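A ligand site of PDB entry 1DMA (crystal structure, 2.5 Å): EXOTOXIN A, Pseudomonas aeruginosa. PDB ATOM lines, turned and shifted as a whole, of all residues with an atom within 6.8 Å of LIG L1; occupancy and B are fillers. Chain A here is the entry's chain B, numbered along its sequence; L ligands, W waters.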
ATOM      1  N   HIS A  41     -29.574 -29.868   7.640  1.00  0.00           N
ATOM      2  CA  HIS A  41     -28.588 -28.838   7.511  1.00  0.00           C
ATOM      3  C   HIS A  41     -27.446 -29.465   6.761  1.00  0.00           C
ATOM      4  O   HIS A  41     -26.842 -30.373   7.281  1.00  0.00           O
ATOM      5  CB  HIS A  41     -28.106 -28.370   8.886  1.00  0.00           C
ATOM      6  CG  HIS A  41     -26.923 -27.467   8.807  1.00  0.00           C
ATOM      7  ND1 HIS A  41     -27.018 -26.138   8.417  1.00  0.00           N
ATOM      8  CD2 HIS A  41     -25.598 -27.717   9.003  1.00  0.00           C
ATOM      9  CE1 HIS A  41     -25.810 -25.617   8.372  1.00  0.00           C
ATOM     10  NE2 HIS A  41     -24.940 -26.546   8.721  1.00  0.00           N
ATOM     11  N   GLY A  42     -27.208 -29.025   5.528  1.00  0.00           N
ATOM     12  CA  GLY A  42     -26.098 -29.555   4.748  1.00  0.00           C
ATOM     13  C   GLY A  42     -24.876 -28.676   4.891  1.00  0.00           C
ATOM     14  O   GLY A  42     -24.999 -27.438   4.827  1.00  0.00           O
ATOM     15  N   THR A  43     -23.732 -29.297   5.188  1.00  0.00           N
ATOM     16  CA  THR A  43     -22.466 -28.612   5.345  1.00  0.00           C
ATOM     17  C   THR A  43     -21.333 -29.581   4.970  1.00  0.00           C
ATOM     18  O   THR A  43     -21.589 -30.690   4.575  1.00  0.00           O
ATOM     19  CB  THR A  43     -22.297 -28.047   6.752  1.00  0.00           C
ATOM     20  OG1 THR A  43     -21.163 -27.160   6.785  1.00  0.00           O
ATOM     21  CG2 THR A  43     -22.102 -29.168   7.741  1.00  0.00           C
ATOM     22  N   PHE A  44     -20.080 -29.131   5.056  1.00  0.00           N
ATOM     23  CA  PHE A  44     -18.913 -29.919   4.666  1.00  0.00           C
ATOM     24  C   PHE A  44     -18.381 -30.734   5.779  1.00  0.00           C
ATOM     25  O   PHE A  44     -18.553 -30.370   6.928  1.00  0.00           O
ATOM     26  CB  PHE A  44     -17.784 -29.012   4.149  1.00  0.00           C
ATOM     27  CG  PHE A  44     -17.374 -27.898   5.102  1.00  0.00           C
ATOM     28  CD1 PHE A  44     -18.103 -26.698   5.141  1.00  0.00           C
ATOM     29  CD2 PHE A  44     -16.311 -28.069   5.988  1.00  0.00           C
ATOM     30  CE1 PHE A  44     -17.781 -25.673   6.039  1.00  0.00           C
ATOM     31  CE2 PHE A  44     -15.963 -27.041   6.911  1.00  0.00           C
ATOM     32  CZ  PHE A  44     -16.717 -25.849   6.934  1.00  0.00           C
ATOM     33  N   GLU A  46     -15.534 -31.309   7.899  1.00  0.00           N
ATOM     34  CA  GLU A  46     -15.086 -30.966   9.228  1.00  0.00           C
ATOM     35  C   GLU A  46     -16.057 -30.073   9.977  1.00  0.00           C
ATOM     36  O   GLU A  46     -16.020 -30.023  11.207  1.00  0.00           O
ATOM     37  CB  GLU A  46     -13.692 -30.390   9.210  1.00  0.00           C
ATOM     38  CG  GLU A  46     -13.456 -29.394   8.092  1.00  0.00           C
ATOM     39  CD  GLU A  46     -13.135 -30.048   6.757  1.00  0.00           C
ATOM     40  OE1 GLU A  46     -12.563 -31.182   6.758  1.00  0.00           O
ATOM     41  OE2 GLU A  46     -13.443 -29.403   5.723  1.00  0.00           O
ATOM     42  N   ALA A  47     -16.976 -29.442   9.254  1.00  0.00           N
ATOM     43  CA  ALA A  47     -17.997 -28.595   9.867  1.00  0.00           C
ATOM     44  C   ALA A  47     -19.023 -29.514  10.454  1.00  0.00           C
ATOM     45  O   ALA A  47     -19.672 -29.156  11.433  1.00  0.00           O
ATOM     46  CB  ALA A  47     -18.656 -27.754   8.886  1.00  0.00           C
ATOM     47  N   ALA A  48     -19.250 -30.663   9.817  1.00  0.00           N
ATOM     48  CA  ALA A  48     -20.207 -31.661  10.324  1.00  0.00           C
ATOM     49  C   ALA A  48     -19.600 -32.252  11.593  1.00  0.00           C
ATOM     50  O   ALA A  48     -20.266 -32.409  12.628  1.00  0.00           O
ATOM     51  CB  ALA A  48     -20.503 -32.774   9.271  1.00  0.00           C
ATOM     52  N   SER A  50     -17.533 -30.877  13.721  1.00  0.00           N
ATOM     53  CA  SER A  50     -17.703 -29.874  14.787  1.00  0.00           C
ATOM     54  C   SER A  50     -19.080 -29.836  15.437  1.00  0.00           C
ATOM     55  O   SER A  50     -19.191 -29.824  16.638  1.00  0.00           O
ATOM     56  CB  SER A  50     -17.397 -28.482  14.214  1.00  0.00           C
ATOM     57  OG  SER A  50     -17.832 -27.437  15.070  1.00  0.00           O
ATOM     58  N   ILE A  51     -20.101 -29.651  14.618  1.00  0.00           N
ATOM     59  CA  ILE A  51     -21.492 -29.559  15.029  1.00  0.00           C
ATOM     60  C   ILE A  51     -21.979 -30.749  15.816  1.00  0.00           C
ATOM     61  O   ILE A  51     -22.695 -30.602  16.815  1.00  0.00           O
ATOM     62  CB  ILE A  51     -22.409 -29.423  13.776  1.00  0.00           C
ATOM     63  CG1 ILE A  51     -22.266 -28.049  13.152  1.00  0.00           C
ATOM     64  CG2 ILE A  51     -23.868 -29.721  14.112  1.00  0.00           C
ATOM     65  CD1 ILE A  51     -23.265 -27.805  12.046  1.00  0.00           C
ATOM     66  N   VAL A  52     -21.681 -31.954  15.305  1.00  0.00           N
ATOM     67  CA  VAL A  52     -22.120 -33.214  15.913  1.00  0.00           C
ATOM     68  C   VAL A  52     -21.386 -33.572  17.197  1.00  0.00           C
ATOM     69  O   VAL A  52     -21.988 -34.004  18.179  1.00  0.00           O
ATOM     70  CB  VAL A  52     -21.984 -34.371  14.927  1.00  0.00           C
ATOM     71  CG1 VAL A  52     -22.383 -35.635  15.565  1.00  0.00           C
ATOM     72  CG2 VAL A  52     -22.868 -34.143  13.745  1.00  0.00           C
ATOM     73  N   GLY A  54     -19.135 -31.313  18.722  1.00  0.00           N
ATOM     74  CA  GLY A  54     -18.855 -30.146  19.537  1.00  0.00           C
ATOM     75  C   GLY A  54     -20.111 -29.312  19.866  1.00  0.00           C
ATOM     76  O   GLY A  54     -20.140 -28.591  20.870  1.00  0.00           O
ATOM     77  N   GLY A  55     -21.139 -29.384  19.034  1.00  0.00           N
ATOM     78  CA  GLY A  55     -22.339 -28.604  19.276  1.00  0.00           C
ATOM     79  C   GLY A  55     -22.426 -27.409  18.342  1.00  0.00           C
ATOM     80  O   GLY A  55     -21.437 -26.995  17.711  1.00  0.00           O
ATOM     81  N   VAL A  56     -23.650 -26.891  18.185  1.00  0.00           N
ATOM     82  CA  VAL A  56     -23.842 -25.741  17.323  1.00  0.00           C
ATOM     83  C   VAL A  56     -23.459 -24.519  18.132  1.00  0.00           C
ATOM     84  O   VAL A  56     -24.000 -24.312  19.220  1.00  0.00           O
ATOM     85  CB  VAL A  56     -25.292 -25.621  16.927  1.00  0.00           C
ATOM     86  CG1 VAL A  56     -25.546 -24.275  16.294  1.00  0.00           C
ATOM     87  CG2 VAL A  56     -25.668 -26.762  15.991  1.00  0.00           C
ATOM     88  N   ARG A  57     -22.510 -23.737  17.614  1.00  0.00           N
ATOM     89  CA  ARG A  57     -22.015 -22.523  18.269  1.00  0.00           C
ATOM     90  C   ARG A  57     -22.005 -21.366  17.208  1.00  0.00           C
ATOM     91  O   ARG A  57     -21.791 -21.621  16.034  1.00  0.00           O
ATOM     92  CB  ARG A  57     -20.668 -22.781  18.975  1.00  0.00           C
ATOM     93  N   ALA A  58     -22.157 -20.123  17.641  1.00  0.00           N
ATOM     94  CA  ALA A  58     -22.287 -18.961  16.747  1.00  0.00           C
ATOM     95  C   ALA A  58     -21.200 -18.189  15.963  1.00  0.00           C
ATOM     96  O   ALA A  58     -21.496 -17.705  14.800  1.00  0.00           O
ATOM     97  CB  ALA A  58     -23.181 -17.925  17.418  1.00  0.00           C
ATOM     98  N   ARG A  59     -20.008 -18.045  16.523  1.00  0.00           N
ATOM     99  CA  ARG A  59     -18.923 -17.243  15.879  1.00  0.00           C
ATOM    100  C   ARG A  59     -18.997 -15.908  16.619  1.00  0.00           C
ATOM    101  O   ARG A  59     -20.035 -15.235  16.614  1.00  0.00           O
ATOM    102  CB  ARG A  59     -19.117 -16.961  14.373  1.00  0.00           C
ATOM    103  CG  ARG A  59     -18.398 -17.898  13.369  1.00  0.00           C
ATOM    104  CD  ARG A  59     -18.651 -17.485  11.856  1.00  0.00           C
ATOM    105  NE  ARG A  59     -18.246 -16.109  11.603  1.00  0.00           N
ATOM    106  CZ  ARG A  59     -19.069 -15.093  11.286  1.00  0.00           C
ATOM    107  NH1 ARG A  59     -20.370 -15.260  11.113  1.00  0.00           N
ATOM    108  NH2 ARG A  59     -18.591 -13.858  11.355  1.00  0.00           N
ATOM    109  N   GLN A  61     -18.180 -13.174  15.897  1.00  0.00           N
ATOM    110  CA  GLN A  61     -18.096 -12.063  14.982  1.00  0.00           C
ATOM    111  C   GLN A  61     -19.483 -11.751  14.423  1.00  0.00           C
ATOM    112  O   GLN A  61     -20.388 -12.569  14.483  1.00  0.00           O
ATOM    113  CB  GLN A  61     -17.129 -12.414  13.849  1.00  0.00           C
ATOM    114  N   ARG A  68     -28.670 -12.819  11.064  1.00  0.00           N
ATOM    115  CA  ARG A  68     -27.819 -13.889  11.573  1.00  0.00           C
ATOM    116  C   ARG A  68     -28.683 -15.039  12.131  1.00  0.00           C
ATOM    117  O   ARG A  68     -29.713 -14.793  12.744  1.00  0.00           O
ATOM    118  CB  ARG A  68     -26.808 -13.332  12.581  1.00  0.00           C
ATOM    119  CG  ARG A  68     -27.429 -12.659  13.742  1.00  0.00           C
ATOM    120  CD  ARG A  68     -26.414 -12.075  14.613  1.00  0.00           C
ATOM    121  NE  ARG A  68     -25.193 -12.874  14.752  1.00  0.00           N
ATOM    122  CZ  ARG A  68     -24.841 -13.534  15.857  1.00  0.00           C
ATOM    123  NH1 ARG A  68     -25.696 -13.633  16.868  1.00  0.00           N
ATOM    124  NH2 ARG A  68     -23.684 -14.182  15.896  1.00  0.00           N
ATOM    125  N   GLY A  69     -28.287 -16.268  11.803  1.00  0.00           N
ATOM    126  CA  GLY A  69     -29.028 -17.455  12.223  1.00  0.00           C
ATOM    127  C   GLY A  69     -28.326 -18.683  11.675  1.00  0.00           C
ATOM    128  O   GLY A  69     -27.276 -18.541  11.066  1.00  0.00           O
ATOM    129  N   PHE A  70     -28.853 -19.899  11.957  1.00  0.00           N
ATOM    130  CA  PHE A  70     -28.323 -21.218  11.515  1.00  0.00           C
ATOM    131  C   PHE A  70     -29.445 -21.689  10.592  1.00  0.00           C
ATOM    132  O   PHE A  70     -30.580 -21.839  11.033  1.00  0.00           O
ATOM    133  CB  PHE A  70     -28.262 -22.186  12.696  1.00  0.00           C
ATOM    134  CG  PHE A  70     -27.575 -23.528  12.398  1.00  0.00           C
ATOM    135  CD1 PHE A  70     -26.211 -23.607  12.165  1.00  0.00           C
ATOM    136  CD2 PHE A  70     -28.294 -24.728  12.508  1.00  0.00           C
ATOM    137  CE1 PHE A  70     -25.591 -24.835  12.066  1.00  0.00           C
ATOM    138  CE2 PHE A  70     -27.690 -25.966  12.403  1.00  0.00           C
ATOM    139  CZ  PHE A  70     -26.351 -26.029  12.182  1.00  0.00           C
ATOM    140  N   TYR A  71     -29.123 -21.837   9.302  1.00  0.00           N
ATOM    141  CA  TYR A  71     -30.066 -22.265   8.267  1.00  0.00           C
ATOM    142  C   TYR A  71     -30.226 -23.751   8.123  1.00  0.00           C
ATOM    143  O   TYR A  71     -29.254 -24.504   8.066  1.00  0.00           O
ATOM    144  CB  TYR A  71     -29.608 -21.766   6.905  1.00  0.00           C
ATOM    145  CG  TYR A  71     -29.888 -20.329   6.609  1.00  0.00           C
ATOM    146  CD1 TYR A  71     -29.061 -19.319   7.098  1.00  0.00           C
ATOM    147  CD2 TYR A  71     -30.920 -19.962   5.766  1.00  0.00           C
ATOM    148  CE1 TYR A  71     -29.257 -17.991   6.762  1.00  0.00           C
ATOM    149  CE2 TYR A  71     -31.113 -18.610   5.421  1.00  0.00           C
ATOM    150  CZ  TYR A  71     -30.283 -17.636   5.923  1.00  0.00           C
ATOM    151  OH  TYR A  71     -30.479 -16.300   5.616  1.00  0.00           O
ATOM    152  N   LEU A 100     -27.061 -33.375   7.975  1.00  0.00           N
ATOM    153  CA  LEU A 100     -27.395 -33.547   9.379  1.00  0.00           C
ATOM    154  C   LEU A 100     -28.855 -33.204   9.562  1.00  0.00           C
ATOM    155  O   LEU A 100     -29.384 -32.327   8.861  1.00  0.00           O
ATOM    156  CB  LEU A 100     -26.609 -32.555  10.219  1.00  0.00           C
ATOM    157  CG  LEU A 100     -25.118 -32.543  10.100  1.00  0.00           C
ATOM    158  CD1 LEU A 100     -24.593 -31.266  10.698  1.00  0.00           C
ATOM    159  CD2 LEU A 100     -24.572 -33.736  10.818  1.00  0.00           C
ATOM    160  N   TRP A 159     -29.597 -17.785  16.544  1.00  0.00           N
ATOM    161  CA  TRP A 159     -28.537 -18.529  17.172  1.00  0.00           C
ATOM    162  C   TRP A 159     -28.797 -19.038  18.600  1.00  0.00           C
ATOM    163  O   TRP A 159     -28.227 -20.060  18.976  1.00  0.00           O
ATOM    164  CB  TRP A 159     -27.248 -17.760  17.071  1.00  0.00           C
ATOM    165  CG  TRP A 159     -26.568 -17.882  15.767  1.00  0.00           C
ATOM    166  CD1 TRP A 159     -26.340 -16.902  14.891  1.00  0.00           C
ATOM    167  CD2 TRP A 159     -25.930 -19.065  15.229  1.00  0.00           C
ATOM    168  NE1 TRP A 159     -25.583 -17.363  13.827  1.00  0.00           N
ATOM    169  CE2 TRP A 159     -25.317 -18.693  14.015  1.00  0.00           C
ATOM    170  CE3 TRP A 159     -25.827 -20.392  15.668  1.00  0.00           C
ATOM    171  CZ2 TRP A 159     -24.593 -19.585  13.220  1.00  0.00           C
ATOM    172  CZ3 TRP A 159     -25.107 -21.296  14.865  1.00  0.00           C
ATOM    173  CH2 TRP A 159     -24.507 -20.881  13.657  1.00  0.00           C
HETATM  174  P1  LIG L   1     -21.955 -18.721  10.245  1.00  0.00           P
HETATM  175  O1  LIG L   1     -23.305 -18.946   9.689  1.00  0.00           O
HETATM  176  O2  LIG L   1     -21.836 -17.701  11.379  1.00  0.00           O
HETATM  177  O3  LIG L   1     -20.953 -18.471   8.954  1.00  0.00           O
HETATM  178  O4  LIG L   1     -21.410 -20.243  10.604  1.00  0.00           O
HETATM  179  C1  LIG L   1     -22.281 -21.321  10.227  1.00  0.00           C
HETATM  180  C2  LIG L   1     -21.748 -22.047   9.024  1.00  0.00           C
HETATM  181  O5  LIG L   1     -20.672 -22.730   9.644  1.00  0.00           O
HETATM  182  C3  LIG L   1     -22.541 -23.197   8.524  1.00  0.00           C
HETATM  183  O6  LIG L   1     -22.030 -23.595   7.263  1.00  0.00           O
HETATM  184  C4  LIG L   1     -22.242 -24.317   9.484  1.00  0.00           C
HETATM  185  O7  LIG L   1     -22.415 -25.557   8.831  1.00  0.00           O
HETATM  186  C5  LIG L   1     -20.775 -24.152   9.659  1.00  0.00           C
HETATM  187  N1  LIG L   1     -20.330 -24.664  10.964  1.00  0.00           N
HETATM  188  C6  LIG L   1     -19.176 -25.285  11.189  1.00  0.00           C
HETATM  189  N2  LIG L   1     -19.026 -25.388  12.516  1.00  0.00           N
HETATM  190  C7  LIG L   1     -20.094 -24.829  13.073  1.00  0.00           C
HETATM  191  C8  LIG L   1     -20.501 -24.970  14.393  1.00  0.00           C
HETATM  192  N3  LIG L   1     -19.775 -25.705  15.236  1.00  0.00           N
HETATM  193  N4  LIG L   1     -21.721 -24.550  14.734  1.00  0.00           N
HETATM  194  C9  LIG L   1     -22.541 -24.050  13.813  1.00  0.00           C
HETATM  195  N5  LIG L   1     -22.167 -23.942  12.545  1.00  0.00           N
HETATM  196  C10 LIG L   1     -20.945 -24.366  12.129  1.00  0.00           C
HETATM  197  N1  LG2 L   2     -29.717 -22.309   3.531  1.00  0.00           N
HETATM  198  C1  LG2 L   2     -28.589 -23.128   3.926  1.00  0.00           C
HETATM  199  C2  LG2 L   2     -28.708 -24.500   4.203  1.00  0.00           C
HETATM  200  C3  LG2 L   2     -29.891 -25.122   4.047  1.00  0.00           C
HETATM  201  C4  LG2 L   2     -30.995 -24.312   3.669  1.00  0.00           C
HETATM  202  C5  LG2 L   2     -30.975 -22.911   3.428  1.00  0.00           C
HETATM  203  C6  LG2 L   2     -27.525 -25.333   4.598  1.00  0.00           C
HETATM  204  O1  LG2 L   2     -27.705 -26.525   4.757  1.00  0.00           O
HETATM  205  N2  LG2 L   2     -26.346 -24.650   4.662  1.00  0.00           N
HETATM  206  O   HOH W   1     -18.733 -26.819  17.672  1.00  0.00           O
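The backbone carbonyl oxygen (O) of Gly 55 lies within hydrogen-bond range of a nitrogen (N3) of LIG L1 (3.2 Å). An oxygen (O7) of LIG L1 sits at hydrogen-bond distance from a ring nitrogen (NE2) of His 41, 2.7 Å away. A nitrogen (N3) of LIG L1 sits at hydrogen-bond distance from the side-chain hydroxyl (OG) of Ser 50, at 2.6 Å. O of Gly 42 is in hydrogen-bond range of N2 of LG2 L2 (3.1 Å). The backbone NH (N) of Gly 42 is in hydrogen-bond range of an oxygen (O1) of LG2 L2, 2.7 Å away. N of Arg 57 lies within hydrogen-bond range of N4 of LIG L1 (3.1 Å). An oxygen (O2) of LIG L1 is in salt-bridge range of the guanidinium group of Arg 59. OG1 of Thr 43 sits at hydrogen-bond distance from O7 of LIG L1 (2.9 Å).
O of Leu 100 lies within hydrogen-bond range of N of His 41 (2.8 Å). O of Gly 69 is in hydrogen-bond range of NE1 of Trp 159 (3.4 Å). A ring nitrogen (ND1) of His 41 sits at hydrogen-bond distance from the backbone carbonyl oxygen of Tyr 71 (2.8 Å). N of Gly 55 is in hydrogen-bond range of O of Ser 50 (3.1 Å).
O2 of LIG L1 lies close to O of Ala 58, at 3.4 Å. Ala 47 touches LIG L1. CG1 of Ile 51 touches C8 of LIG L1, 3.8 Å away. Val 56 touches LIG L1. Phe 70 touches LIG L1. Trp 159 touches LIG L1. Hydrophobic or aromatic side chains within 4 Å of LIG L1: His 41, Ala 47, Ile 51, Val 56, Phe 70 and Trp 159. Of the 23 residues printed, 12 come within 4 Å of LIG L1. Along chain A the residues within 4 Å of LIG L1 span positions 41 to 159. The nearest printed residue that does not touch LIG L1 is Gly 69 (4.2 Å).
Water W1 lies within hydrogen-bond range of O of Gly 55 (2.7 Å), OG of Ser 50 (2.8 Å) and N3 of LIG L1 (2.9 Å).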
